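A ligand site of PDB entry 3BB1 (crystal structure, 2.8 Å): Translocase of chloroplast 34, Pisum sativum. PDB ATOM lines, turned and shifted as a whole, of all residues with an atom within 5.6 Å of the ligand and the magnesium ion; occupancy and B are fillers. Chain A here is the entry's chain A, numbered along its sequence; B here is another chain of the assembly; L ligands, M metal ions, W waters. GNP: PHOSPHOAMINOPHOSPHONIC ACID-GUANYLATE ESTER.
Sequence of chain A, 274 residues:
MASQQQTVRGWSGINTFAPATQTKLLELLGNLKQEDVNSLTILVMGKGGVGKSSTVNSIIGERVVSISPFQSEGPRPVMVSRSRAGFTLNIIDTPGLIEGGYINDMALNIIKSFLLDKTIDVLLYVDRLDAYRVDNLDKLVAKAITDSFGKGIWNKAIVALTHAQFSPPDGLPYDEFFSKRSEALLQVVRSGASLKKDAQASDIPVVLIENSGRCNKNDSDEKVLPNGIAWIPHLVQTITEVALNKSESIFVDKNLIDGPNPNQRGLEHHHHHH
Water W2 bridges an oxygen (O2A) of the ligand (2.5 Å) and the backbone carbonyl oxygen (O) of Ser 66 (2.8 Å). Water W3 bridges O of Thr 94 and OD1 of Asp 93. Water W4 lies within hydrogen-bond range of OE1 of Glu 210, N2 of the ligand and NH2 of Arg 214.
The magnesium ion is bound by OG of Ser 53 (1.9 Å). The magnesium ion is bound by O2G of the ligand (2.0 Å). The magnesium ion is bound by O2B of the ligand (2.0 Å). Water W3 binds the magnesium ion, at 2.1 Å. Water W1 binds the magnesium ion (2.1 Å). The magnesium ion is bound by water W2, 2.1 Å away. The magnesium ion has six donor atoms within binding distance.
An oxygen (O1A) of the ligand lies close to the backbone NH (N) of Ser 53 (3.3 Å). O1B of the ligand lies within hydrogen-bond range of N of Lys 52 (2.7 Å). The side-chain amino group (NZ) of Lys 52 lies within salt-bridge range of an oxygen (O1B) of the ligand (2.5 Å). NH2 of Arg 133 of chain B lies within salt-bridge range of O1G of the ligand, 2.6 Å away. O1G of the ligand sits close to O of Ser 72, 2.7 Å away. The backbone NH (N) of Asn 211 sits at hydrogen-bond distance from an oxygen (O6) of the ligand (2.7 Å). ND2 of Asn 211 is in hydrogen-bond range of N7 of the ligand, 3.2 Å away. The backbone NH (N) of Gly 51 sits at hydrogen-bond distance from an oxygen (O1B) of the ligand (2.8 Å). The side-chain carboxylate (OE2) of Glu 210 is in hydrogen-bond range of a nitrogen (N1) of the ligand. N of Ser 54 sits at hydrogen-bond distance from O1A of the ligand, 2.8 Å away. The side-chain hydroxyl (OG) of Ser 54 sits at hydrogen-bond distance from an oxygen (O1A) of the ligand (2.8 Å). The backbone NH of His 163 lies within hydrogen-bond range of an oxygen (O6) of the ligand (3.0 Å). NE2 of His 163 sits at hydrogen-bond distance from N3 of the ligand (3.2 Å). O2A of the ligand lies within hydrogen-bond range of N of Ser 68, 3.0 Å away. N of Gly 49 is in hydrogen-bond range of O3G of the ligand. The side-chain carboxylate (OD1) of Asp 170 of chain B is in hydrogen-bond range of an oxygen (O2') of the ligand (3.1 Å). N of Val 50 is in hydrogen-bond range of O1B of the ligand. N of Gly 96 is in hydrogen-bond range of O3G of the ligand.
Merely in contact with the magnesium ion: Asp 93 (3.8 Å). Along chain A the residues within 4 Å of the magnesium ion span positions 53 to 93.
The side-chain hydroxyl (OG) of Ser 53 sits close to the side-chain carboxylate (OD2) of Asp 93 (2.6 Å). The side-chain hydroxyl of Ser 53 sits close to the backbone carbonyl oxygen of Ser 66 (3.3 Å). NH2 of Arg 133 of chain B sits close to OG of Ser 72 (3.5 Å). NH1 of Arg 133 of chain B lies within hydrogen-bond range of O of Ser 68, at 3.0 Å. The side-chain hydroxyl of Thr 55 lies within hydrogen-bond range of the backbone carbonyl oxygen of Gly 51 (2.8 Å). The side-chain carboxylate of Glu 210 lies within hydrogen-bond range of the backbone NH of Ala 164. The backbone NH (N) of His 163 is in hydrogen-bond range of the backbone carbonyl oxygen (O) of Ile 209 (3.2 Å). The backbone NH (N) of Glu 73 lies within hydrogen-bond range of the side-chain hydroxyl (OG) of Ser 68, at 3.2 Å.
CA of Gly 48 touches O3G of the ligand (3.2 Å). Ile 67 touches the ligand (CG2 to C3', 3.9 Å). Pro 69 touches the ligand (CB to O3', 3.4 Å). CB of Thr 162 touches O6 of the ligand, 3.7 Å away. Ile 209 touches the ligand. Arg 214 touches the ligand (NH2 to N2, 3.9 Å). Tyr 132 of chain B touches the ligand (CE2 to O4', 3.1 Å). CB of Pro 169 of chain B touches O2' of the ligand, 3.0 Å away. Hydrophobic or aromatic side chains that line the ligand: Val 50, Ile 67, Pro 69, His 163, Tyr 132 of chain B and Pro 169 of chain B. 22 residues have an atom within 4 Å of the ligand: Gly 48, Gly 49, Val 50, Gly 51, Lys 52, Ser 53, Ser 54, Ile 67, Ser 68, Pro 69, Ser 72, Gly 96, Thr 162, His 163, Ile 209, Glu 210, Asn 211, Arg 214, Tyr 132 of chain B, Arg 133 of chain B, Pro 169 of chain B and Asp 170 of chain B.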
ATOM      1  N   LYS A  47     -17.751 -32.033 -18.686  1.00  0.00           N
ATOM      2  CA  LYS A  47     -17.718 -32.180 -17.229  1.00  0.00           C
ATOM      3  C   LYS A  47     -18.204 -30.888 -16.577  1.00  0.00           C
ATOM      4  O   LYS A  47     -18.313 -29.836 -17.222  1.00  0.00           O
ATOM      5  CB  LYS A  47     -16.297 -32.517 -16.779  1.00  0.00           C
ATOM      6  CG  LYS A  47     -15.881 -33.935 -17.145  1.00  0.00           C
ATOM      7  CD  LYS A  47     -14.574 -34.324 -16.470  1.00  0.00           C
ATOM      8  CE  LYS A  47     -13.474 -33.246 -16.640  1.00  0.00           C
ATOM      9  NZ  LYS A  47     -12.121 -33.755 -16.259  1.00  0.00           N
ATOM     10  N   GLY A  48     -18.536 -30.954 -15.323  1.00  0.00           N
ATOM     11  CA  GLY A  48     -19.069 -29.786 -14.687  1.00  0.00           C
ATOM     12  C   GLY A  48     -17.943 -28.878 -14.280  1.00  0.00           C
ATOM     13  O   GLY A  48     -16.826 -29.330 -14.070  1.00  0.00           O
ATOM     14  N   GLY A  49     -18.222 -27.589 -14.182  1.00  0.00           N
ATOM     15  CA  GLY A  49     -17.230 -26.627 -13.704  1.00  0.00           C
ATOM     16  C   GLY A  49     -16.081 -26.352 -14.647  1.00  0.00           C
ATOM     17  O   GLY A  49     -15.050 -25.880 -14.221  1.00  0.00           O
ATOM     18  N   VAL A  50     -16.245 -26.617 -15.925  1.00  0.00           N
ATOM     19  CA  VAL A  50     -15.186 -26.350 -16.891  1.00  0.00           C
ATOM     20  C   VAL A  50     -15.311 -25.062 -17.699  1.00  0.00           C
ATOM     21  O   VAL A  50     -14.372 -24.732 -18.458  1.00  0.00           O
ATOM     22  CB  VAL A  50     -15.044 -27.499 -17.896  1.00  0.00           C
ATOM     23  CG1 VAL A  50     -14.893 -28.820 -17.106  1.00  0.00           C
ATOM     24  CG2 VAL A  50     -16.215 -27.474 -18.959  1.00  0.00           C
ATOM     25  N   GLY A  51     -16.439 -24.330 -17.540  1.00  0.00           N
ATOM     26  CA  GLY A  51     -16.702 -23.120 -18.362  1.00  0.00           C
ATOM     27  C   GLY A  51     -17.601 -23.236 -19.605  1.00  0.00           C
ATOM     28  O   GLY A  51     -17.575 -22.367 -20.498  1.00  0.00           O
ATOM     29  N   LYS A  52     -18.422 -24.304 -19.657  1.00  0.00           N
ATOM     30  CA  LYS A  52     -19.497 -24.383 -20.643  1.00  0.00           C
ATOM     31  C   LYS A  52     -20.296 -23.041 -20.699  1.00  0.00           C
ATOM     32  O   LYS A  52     -20.420 -22.448 -21.749  1.00  0.00           O
ATOM     33  CB  LYS A  52     -20.432 -25.551 -20.342  1.00  0.00           C
ATOM     34  CG  LYS A  52     -19.837 -26.949 -20.509  1.00  0.00           C
ATOM     35  CD  LYS A  52     -20.764 -28.063 -19.995  1.00  0.00           C
ATOM     36  CE  LYS A  52     -21.216 -27.892 -18.546  1.00  0.00           C
ATOM     37  NZ  LYS A  52     -20.076 -27.722 -17.634  1.00  0.00           N
ATOM     38  N   SER A  53     -20.809 -22.582 -19.565  1.00  0.00           N
ATOM     39  CA  SER A  53     -21.692 -21.431 -19.544  1.00  0.00           C
ATOM     40  C   SER A  53     -20.971 -20.136 -19.940  1.00  0.00           C
ATOM     41  O   SER A  53     -21.514 -19.294 -20.684  1.00  0.00           O
ATOM     42  CB  SER A  53     -22.322 -21.291 -18.159  1.00  0.00           C
ATOM     43  OG  SER A  53     -23.129 -22.414 -17.827  1.00  0.00           O
ATOM     44  N   SER A  54     -19.746 -19.999 -19.442  1.00  0.00           N
ATOM     45  CA  SER A  54     -18.885 -18.846 -19.649  1.00  0.00           C
ATOM     46  C   SER A  54     -18.545 -18.651 -21.116  1.00  0.00           C
ATOM     47  O   SER A  54     -18.559 -17.544 -21.611  1.00  0.00           O
ATOM     48  CB  SER A  54     -17.600 -18.997 -18.836  1.00  0.00           C
ATOM     49  OG  SER A  54     -17.857 -18.880 -17.437  1.00  0.00           O
ATOM     50  N   THR A  55     -18.178 -19.763 -21.772  1.00  0.00           N
ATOM     51  CA  THR A  55     -18.001 -19.859 -23.223  1.00  0.00           C
ATOM     52  C   THR A  55     -19.266 -19.482 -23.981  1.00  0.00           C
ATOM     53  O   THR A  55     -19.190 -18.718 -24.929  1.00  0.00           O
ATOM     54  CB  THR A  55     -17.582 -21.308 -23.625  1.00  0.00           C
ATOM     55  OG1 THR A  55     -16.377 -21.617 -22.948  1.00  0.00           O
ATOM     56  CG2 THR A  55     -17.321 -21.476 -25.115  1.00  0.00           C
ATOM     57  N   SER A  66     -26.011 -18.557 -16.763  1.00  0.00           N
ATOM     58  CA  SER A  66     -25.456 -18.252 -15.459  1.00  0.00           C
ATOM     59  C   SER A  66     -24.139 -18.957 -15.181  1.00  0.00           C
ATOM     60  O   SER A  66     -23.808 -19.978 -15.773  1.00  0.00           O
ATOM     61  CB  SER A  66     -26.494 -18.574 -14.396  1.00  0.00           C
ATOM     62  OG  SER A  66     -27.694 -17.895 -14.771  1.00  0.00           O
ATOM     63  N   ILE A  67     -23.405 -18.372 -14.252  1.00  0.00           N
ATOM     64  CA  ILE A  67     -22.037 -18.757 -13.981  1.00  0.00           C
ATOM     65  C   ILE A  67     -21.955 -19.346 -12.597  1.00  0.00           C
ATOM     66  O   ILE A  67     -22.678 -18.952 -11.705  1.00  0.00           O
ATOM     67  CB  ILE A  67     -21.111 -17.542 -14.102  1.00  0.00           C
ATOM     68  CG1 ILE A  67     -20.553 -17.489 -15.514  1.00  0.00           C
ATOM     69  CG2 ILE A  67     -19.944 -17.648 -13.158  1.00  0.00           C
ATOM     70  CD1 ILE A  67     -21.567 -17.286 -16.544  1.00  0.00           C
ATOM     71  N   SER A  68     -21.023 -20.278 -12.420  1.00  0.00           N
ATOM     72  CA  SER A  68     -21.003 -21.104 -11.214  1.00  0.00           C
ATOM     73  C   SER A  68     -19.620 -21.476 -10.678  1.00  0.00           C
ATOM     74  O   SER A  68     -19.100 -22.563 -10.958  1.00  0.00           O
ATOM     75  CB  SER A  68     -21.853 -22.327 -11.475  1.00  0.00           C
ATOM     76  OG  SER A  68     -22.913 -22.298 -10.534  1.00  0.00           O
ATOM     77  N   PRO A  69     -19.050 -20.586  -9.848  1.00  0.00           N
ATOM     78  CA  PRO A  69     -17.695 -20.698  -9.316  1.00  0.00           C
ATOM     79  C   PRO A  69     -17.576 -21.682  -8.161  1.00  0.00           C
ATOM     80  O   PRO A  69     -16.466 -21.941  -7.702  1.00  0.00           O
ATOM     81  CB  PRO A  69     -17.382 -19.275  -8.824  1.00  0.00           C
ATOM     82  CG  PRO A  69     -18.700 -18.626  -8.642  1.00  0.00           C
ATOM     83  CD  PRO A  69     -19.743 -19.371  -9.383  1.00  0.00           C
ATOM     84  N   GLN A  71     -20.650 -24.057  -7.600  1.00  0.00           N
ATOM     85  CA  GLN A  71     -21.988 -24.326  -7.181  1.00  0.00           C
ATOM     86  C   GLN A  71     -22.842 -25.326  -7.918  1.00  0.00           C
ATOM     87  O   GLN A  71     -23.692 -25.936  -7.282  1.00  0.00           O
ATOM     88  CB  GLN A  71     -22.746 -22.999  -6.815  1.00  0.00           C
ATOM     89  CG  GLN A  71     -22.333 -21.649  -7.512  1.00  0.00           C
ATOM     90  CD  GLN A  71     -22.620 -20.379  -6.639  1.00  0.00           C
ATOM     91  OE1 GLN A  71     -22.657 -20.441  -5.398  1.00  0.00           O
ATOM     92  NE2 GLN A  71     -22.838 -19.239  -7.305  1.00  0.00           N
ATOM     93  N   SER A  72     -22.575 -25.583  -9.205  1.00  0.00           N
ATOM     94  CA  SER A  72     -23.548 -26.201 -10.175  1.00  0.00           C
ATOM     95  C   SER A  72     -24.284 -25.112 -10.987  1.00  0.00           C
ATOM     96  O   SER A  72     -23.917 -24.886 -12.164  1.00  0.00           O
ATOM     97  CB  SER A  72     -24.430 -27.336  -9.633  1.00  0.00           C
ATOM     98  OG  SER A  72     -23.675 -28.550  -9.659  1.00  0.00           O
ATOM     99  N   GLU A  73     -25.328 -24.459 -10.477  1.00  0.00           N
ATOM    100  CA  GLU A  73     -26.452 -25.060  -9.828  1.00  0.00           C
ATOM    101  C   GLU A  73     -27.262 -25.815 -10.920  1.00  0.00           C
ATOM    102  O   GLU A  73     -27.612 -26.987 -10.778  1.00  0.00           O
ATOM    103  CB  GLU A  73     -27.341 -23.933  -9.229  1.00  0.00           C
ATOM    104  CG  GLU A  73     -28.013 -22.989 -10.294  1.00  0.00           C
ATOM    105  CD  GLU A  73     -28.530 -21.675  -9.722  1.00  0.00           C
ATOM    106  OE1 GLU A  73     -28.099 -21.293  -8.610  1.00  0.00           O
ATOM    107  OE2 GLU A  73     -29.363 -21.004 -10.380  1.00  0.00           O
ATOM    108  N   GLY A  74     -27.461 -25.122 -12.042  1.00  0.00           N
ATOM    109  CA  GLY A  74     -28.631 -25.283 -12.937  1.00  0.00           C
ATOM    110  C   GLY A  74     -28.687 -26.488 -13.852  1.00  0.00           C
ATOM    111  O   GLY A  74     -28.002 -26.518 -14.889  1.00  0.00           O
ATOM    112  N   ASP A  93     -26.482 -24.553 -24.025  1.00  0.00           N
ATOM    113  CA  ASP A  93     -25.624 -24.729 -22.862  1.00  0.00           C
ATOM    114  C   ASP A  93     -26.234 -25.942 -22.192  1.00  0.00           C
ATOM    115  O   ASP A  93     -27.415 -26.199 -22.362  1.00  0.00           O
ATOM    116  CB  ASP A  93     -25.639 -23.469 -21.958  1.00  0.00           C
ATOM    117  CG  ASP A  93     -24.608 -23.517 -20.769  1.00  0.00           C
ATOM    118  OD1 ASP A  93     -23.669 -24.356 -20.731  1.00  0.00           O
ATOM    119  OD2 ASP A  93     -24.738 -22.686 -19.838  1.00  0.00           O
ATOM    120  N   THR A  94     -25.438 -26.717 -21.469  1.00  0.00           N
ATOM    121  CA  THR A  94     -25.895 -27.973 -20.824  1.00  0.00           C
ATOM    122  C   THR A  94     -25.204 -28.157 -19.470  1.00  0.00           C
ATOM    123  O   THR A  94     -24.133 -27.617 -19.241  1.00  0.00           O
ATOM    124  CB  THR A  94     -25.554 -29.217 -21.666  1.00  0.00           C
ATOM    125  OG1 THR A  94     -24.142 -29.271 -21.793  1.00  0.00           O
ATOM    126  CG2 THR A  94     -26.200 -29.181 -23.051  1.00  0.00           C
ATOM    127  N   PRO A  95     -25.830 -28.926 -18.563  1.00  0.00           N
ATOM    128  CA  PRO A  95     -25.196 -29.212 -17.287  1.00  0.00           C
ATOM    129  C   PRO A  95     -24.035 -30.227 -17.370  1.00  0.00           C
ATOM    130  O   PRO A  95     -24.061 -31.139 -18.173  1.00  0.00           O
ATOM    131  CB  PRO A  95     -26.342 -29.769 -16.440  1.00  0.00           C
ATOM    132  CG  PRO A  95     -27.396 -30.150 -17.374  1.00  0.00           C
ATOM    133  CD  PRO A  95     -27.161 -29.539 -18.696  1.00  0.00           C
ATOM    134  N   GLY A  96     -23.011 -30.052 -16.553  1.00  0.00           N
ATOM    135  CA  GLY A  96     -21.908 -30.990 -16.551  1.00  0.00           C
ATOM    136  C   GLY A  96     -22.410 -32.417 -16.417  1.00  0.00           C
ATOM    137  O   GLY A  96     -23.219 -32.713 -15.551  1.00  0.00           O
ATOM    138  N   THR A 162     -10.519 -24.303 -21.792  1.00  0.00           N
ATOM    139  CA  THR A 162     -10.681 -22.987 -21.248  1.00  0.00           C
ATOM    140  C   THR A 162      -9.536 -22.632 -20.306  1.00  0.00           C
ATOM    141  O   THR A 162      -8.564 -23.368 -20.208  1.00  0.00           O
ATOM    142  CB  THR A 162     -12.074 -22.833 -20.583  1.00  0.00           C
ATOM    143  OG1 THR A 162     -12.172 -23.618 -19.364  1.00  0.00           O
ATOM    144  CG2 THR A 162     -13.116 -23.253 -21.612  1.00  0.00           C
ATOM    145  N   HIS A 163      -9.650 -21.488 -19.640  1.00  0.00           N
ATOM    146  CA  HIS A 163      -8.542 -20.861 -18.931  1.00  0.00           C
ATOM    147  C   HIS A 163      -7.203 -20.867 -19.696  1.00  0.00           C
ATOM    148  O   HIS A 163      -6.132 -21.091 -19.130  1.00  0.00           O
ATOM    149  CB  HIS A 163      -8.330 -21.509 -17.588  1.00  0.00           C
ATOM    150  CG  HIS A 163      -9.544 -21.601 -16.744  1.00  0.00           C
ATOM    151  ND1 HIS A 163     -10.716 -22.153 -17.197  1.00  0.00           N
ATOM    152  CD2 HIS A 163      -9.734 -21.318 -15.430  1.00  0.00           C
ATOM    153  CE1 HIS A 163     -11.601 -22.167 -16.204  1.00  0.00           C
ATOM    154  NE2 HIS A 163     -11.034 -21.659 -15.124  1.00  0.00           N
ATOM    155  N   ALA A 164      -7.283 -20.553 -20.988  1.00  0.00           N
ATOM    156  CA  ALA A 164      -6.144 -20.483 -21.868  1.00  0.00           C
ATOM    157  C   ALA A 164      -5.090 -19.502 -21.395  1.00  0.00           C
ATOM    158  O   ALA A 164      -3.943 -19.665 -21.709  1.00  0.00           O
ATOM    159  CB  ALA A 164      -6.611 -20.135 -23.254  1.00  0.00           C
ATOM    160  N   ILE A 209      -9.545 -21.215 -25.163  1.00  0.00           N
ATOM    161  CA  ILE A 209     -10.555 -20.252 -24.752  1.00  0.00           C
ATOM    162  C   ILE A 209     -10.092 -19.605 -23.470  1.00  0.00           C
ATOM    163  O   ILE A 209      -9.598 -20.250 -22.583  1.00  0.00           O
ATOM    164  CB  ILE A 209     -11.959 -20.924 -24.590  1.00  0.00           C
ATOM    165  CG1 ILE A 209     -12.545 -21.190 -25.979  1.00  0.00           C
ATOM    166  CG2 ILE A 209     -12.933 -20.051 -23.723  1.00  0.00           C
ATOM    167  CD1 ILE A 209     -13.784 -21.998 -25.962  1.00  0.00           C
ATOM    168  N   GLU A 210     -10.224 -18.297 -23.382  1.00  0.00           N
ATOM    169  CA  GLU A 210     -10.002 -17.630 -22.116  1.00  0.00           C
ATOM    170  C   GLU A 210     -11.148 -16.677 -21.919  1.00  0.00           C
ATOM    171  O   GLU A 210     -11.212 -15.629 -22.540  1.00  0.00           O
ATOM    172  CB  GLU A 210      -8.666 -16.891 -22.109  1.00  0.00           C
ATOM    173  CG  GLU A 210      -8.419 -16.067 -20.912  1.00  0.00           C
ATOM    174  CD  GLU A 210      -8.647 -16.827 -19.623  1.00  0.00           C
ATOM    175  OE1 GLU A 210      -7.771 -17.639 -19.224  1.00  0.00           O
ATOM    176  OE2 GLU A 210      -9.694 -16.561 -18.994  1.00  0.00           O
ATOM    177  N   ASN A 211     -12.049 -17.036 -21.033  1.00  0.00           N
ATOM    178  CA  ASN A 211     -13.230 -16.224 -20.879  1.00  0.00           C
ATOM    179  C   ASN A 211     -13.076 -14.984 -20.029  1.00  0.00           C
ATOM    180  O   ASN A 211     -13.980 -14.180 -19.991  1.00  0.00           O
ATOM    181  CB  ASN A 211     -14.354 -17.079 -20.405  1.00  0.00           C
ATOM    182  CG  ASN A 211     -14.782 -18.052 -21.433  1.00  0.00           C
ATOM    183  OD1 ASN A 211     -15.116 -17.678 -22.565  1.00  0.00           O
ATOM    184  ND2 ASN A 211     -14.798 -19.313 -21.066  1.00  0.00           N
ATOM    185  N   SER A 212     -11.916 -14.795 -19.402  1.00  0.00           N
ATOM    186  CA  SER A 212     -11.786 -13.759 -18.378  1.00  0.00           C
ATOM    187  C   SER A 212     -11.831 -12.348 -18.940  1.00  0.00           C
ATOM    188  O   SER A 212     -11.307 -12.068 -20.027  1.00  0.00           O
ATOM    189  CB  SER A 212     -10.494 -13.936 -17.553  1.00  0.00           C
ATOM    190  OG  SER A 212     -10.503 -13.081 -16.395  1.00  0.00           O
ATOM    191  N   ARG A 214     -10.036 -10.110 -17.811  1.00  0.00           N
ATOM    192  CA  ARG A 214      -8.647  -9.663 -17.736  1.00  0.00           C
ATOM    193  C   ARG A 214      -7.747 -10.420 -18.736  1.00  0.00           C
ATOM    194  O   ARG A 214      -6.518 -10.465 -18.599  1.00  0.00           O
ATOM    195  CB  ARG A 214      -8.150  -9.771 -16.262  1.00  0.00           C
ATOM    196  CG  ARG A 214      -7.640 -11.150 -15.895  1.00  0.00           C
ATOM    197  CD  ARG A 214      -7.582 -11.541 -14.393  1.00  0.00           C
ATOM    198  NE  ARG A 214      -7.634 -13.000 -14.188  1.00  0.00           N
ATOM    199  CZ  ARG A 214      -7.063 -13.961 -14.958  1.00  0.00           C
ATOM    200  NH1 ARG A 214      -6.318 -13.677 -16.024  1.00  0.00           N
ATOM    201  NH2 ARG A 214      -7.215 -15.244 -14.648  1.00  0.00           N
ATOM    202  N   TYR B 132     -13.494 -25.393  -8.454  1.00  0.00           N
ATOM    203  CA  TYR B 132     -14.772 -24.755  -8.275  1.00  0.00           C
ATOM    204  C   TYR B 132     -15.781 -25.681  -7.552  1.00  0.00           C
ATOM    205  O   TYR B 132     -16.915 -25.273  -7.303  1.00  0.00           O
ATOM    206  CB  TYR B 132     -15.280 -24.289  -9.632  1.00  0.00           C
ATOM    207  CG  TYR B 132     -14.307 -23.436 -10.436  1.00  0.00           C
ATOM    208  CD1 TYR B 132     -13.671 -22.337  -9.890  1.00  0.00           C
ATOM    209  CD2 TYR B 132     -14.041 -23.732 -11.765  1.00  0.00           C
ATOM    210  CE1 TYR B 132     -12.786 -21.539 -10.670  1.00  0.00           C
ATOM    211  CE2 TYR B 132     -13.152 -22.965 -12.545  1.00  0.00           C
ATOM    212  CZ  TYR B 132     -12.534 -21.874 -12.010  1.00  0.00           C
ATOM    213  OH  TYR B 132     -11.683 -21.127 -12.824  1.00  0.00           O
ATOM    214  N   ARG B 133     -15.388 -26.894  -7.171  1.00  0.00           N
ATOM    215  CA  ARG B 133     -16.335 -27.877  -6.603  1.00  0.00           C
ATOM    216  C   ARG B 133     -15.852 -28.629  -5.353  1.00  0.00           C
ATOM    217  O   ARG B 133     -14.727 -28.552  -4.951  1.00  0.00           O
ATOM    218  CB  ARG B 133     -16.726 -28.922  -7.663  1.00  0.00           C
ATOM    219  CG  ARG B 133     -16.843 -28.401  -9.056  1.00  0.00           C
ATOM    220  CD  ARG B 133     -17.840 -27.276  -9.108  1.00  0.00           C
ATOM    221  NE  ARG B 133     -19.040 -27.649  -9.812  1.00  0.00           N
ATOM    222  CZ  ARG B 133     -19.702 -26.860 -10.644  1.00  0.00           C
ATOM    223  NH1 ARG B 133     -19.309 -25.594 -10.902  1.00  0.00           N
ATOM    224  NH2 ARG B 133     -20.784 -27.356 -11.226  1.00  0.00           N
ATOM    225  N   PRO B 169     -12.152 -15.750 -10.417  1.00  0.00           N
ATOM    226  CA  PRO B 169     -13.030 -15.353 -11.518  1.00  0.00           C
ATOM    227  C   PRO B 169     -13.986 -14.226 -11.174  1.00  0.00           C
ATOM    228  O   PRO B 169     -13.841 -13.591 -10.147  1.00  0.00           O
ATOM    229  CB  PRO B 169     -13.786 -16.654 -11.818  1.00  0.00           C
ATOM    230  CG  PRO B 169     -13.090 -17.730 -11.026  1.00  0.00           C
ATOM    231  CD  PRO B 169     -12.567 -17.035  -9.852  1.00  0.00           C
ATOM    232  N   ASP B 170     -14.996 -14.012 -12.024  1.00  0.00           N
ATOM    233  CA  ASP B 170     -15.750 -12.745 -12.054  1.00  0.00           C
ATOM    234  C   ASP B 170     -15.641 -11.822 -10.847  1.00  0.00           C
ATOM    235  O   ASP B 170     -16.574 -11.597 -10.071  1.00  0.00           O
ATOM    236  CB  ASP B 170     -17.178 -12.779 -12.724  1.00  0.00           C
ATOM    237  CG  ASP B 170     -17.689 -14.203 -13.124  1.00  0.00           C
ATOM    238  OD1 ASP B 170     -17.244 -15.245 -12.519  1.00  0.00           O
ATOM    239  OD2 ASP B 170     -18.580 -14.190 -14.061  1.00  0.00           O
HETATM  240  PG  GNP L   1     -21.586 -26.198 -14.789  1.00  0.00           P
HETATM  241  O1G GNP L   1     -21.857 -26.115 -13.307  1.00  0.00           O
HETATM  242  O2G GNP L   1     -22.716 -25.430 -15.458  1.00  0.00           O
HETATM  243  O3G GNP L   1     -21.363 -27.582 -15.275  1.00  0.00           O
HETATM  244  N3B GNP L   1     -20.148 -25.318 -14.981  1.00  0.00           N
HETATM  245  PB  GNP L   1     -19.684 -24.661 -16.411  1.00  0.00           P
HETATM  246  O1B GNP L   1     -18.911 -25.529 -17.310  1.00  0.00           O
HETATM  247  O2B GNP L   1     -20.831 -23.953 -17.079  1.00  0.00           O
HETATM  248  O3A GNP L   1     -18.588 -23.567 -15.963  1.00  0.00           O
HETATM  249  PA  GNP L   1     -19.027 -22.028 -15.688  1.00  0.00           P
HETATM  250  O1A GNP L   1     -19.263 -21.288 -16.962  1.00  0.00           O
HETATM  251  O2A GNP L   1     -20.070 -22.112 -14.642  1.00  0.00           O
HETATM  252  O5' GNP L   1     -17.701 -21.408 -15.161  1.00  0.00           O
HETATM  253  C5' GNP L   1     -17.057 -22.110 -14.098  1.00  0.00           C
HETATM  254  C4' GNP L   1     -16.178 -21.178 -13.326  1.00  0.00           C
HETATM  255  O4' GNP L   1     -14.981 -21.110 -14.140  1.00  0.00           O
HETATM  256  C3' GNP L   1     -16.684 -19.756 -13.140  1.00  0.00           C
HETATM  257  O3' GNP L   1     -16.083 -19.213 -11.963  1.00  0.00           O
HETATM  258  C2' GNP L   1     -16.073 -18.980 -14.244  1.00  0.00           C
HETATM  259  O2' GNP L   1     -15.791 -17.642 -13.859  1.00  0.00           O
HETATM  260  C1' GNP L   1     -14.753 -19.752 -14.470  1.00  0.00           C
HETATM  261  N9  GNP L   1     -14.275 -19.778 -15.832  1.00  0.00           N
HETATM  262  C8  GNP L   1     -14.885 -20.331 -16.946  1.00  0.00           C
HETATM  263  N7  GNP L   1     -14.203 -20.192 -18.044  1.00  0.00           N
HETATM  264  C5  GNP L   1     -13.056 -19.535 -17.597  1.00  0.00           C
HETATM  265  C6  GNP L   1     -11.925 -19.138 -18.339  1.00  0.00           C
HETATM  266  O6  GNP L   1     -11.690 -19.263 -19.564  1.00  0.00           O
HETATM  267  N1  GNP L   1     -11.026 -18.475 -17.501  1.00  0.00           N
HETATM  268  C2  GNP L   1     -11.134 -18.249 -16.162  1.00  0.00           C
HETATM  269  N2  GNP L   1     -10.121 -17.604 -15.570  1.00  0.00           N
HETATM  270  N3  GNP L   1     -12.177 -18.661 -15.465  1.00  0.00           N
HETATM  271  C4  GNP L   1     -13.082 -19.262 -16.266  1.00  0.00           C
HETATM  272 MG    MG M   1     -22.836 -23.924 -16.764  1.00  0.00          MG
HETATM  273  O   HOH W   1     -24.875 -23.888 -16.365  1.00  0.00           O
HETATM  274  O   HOH W   2     -22.491 -22.440 -15.330  1.00  0.00           O
HETATM  275  O   HOH W   3     -23.165 -25.317 -18.242  1.00  0.00           O
HETATM  276  O   HOH W   4      -7.285 -17.537 -16.824  1.00  0.00           O
HETATM  277  O   HOH W   5     -25.457 -26.430 -15.113  1.00  0.00           O
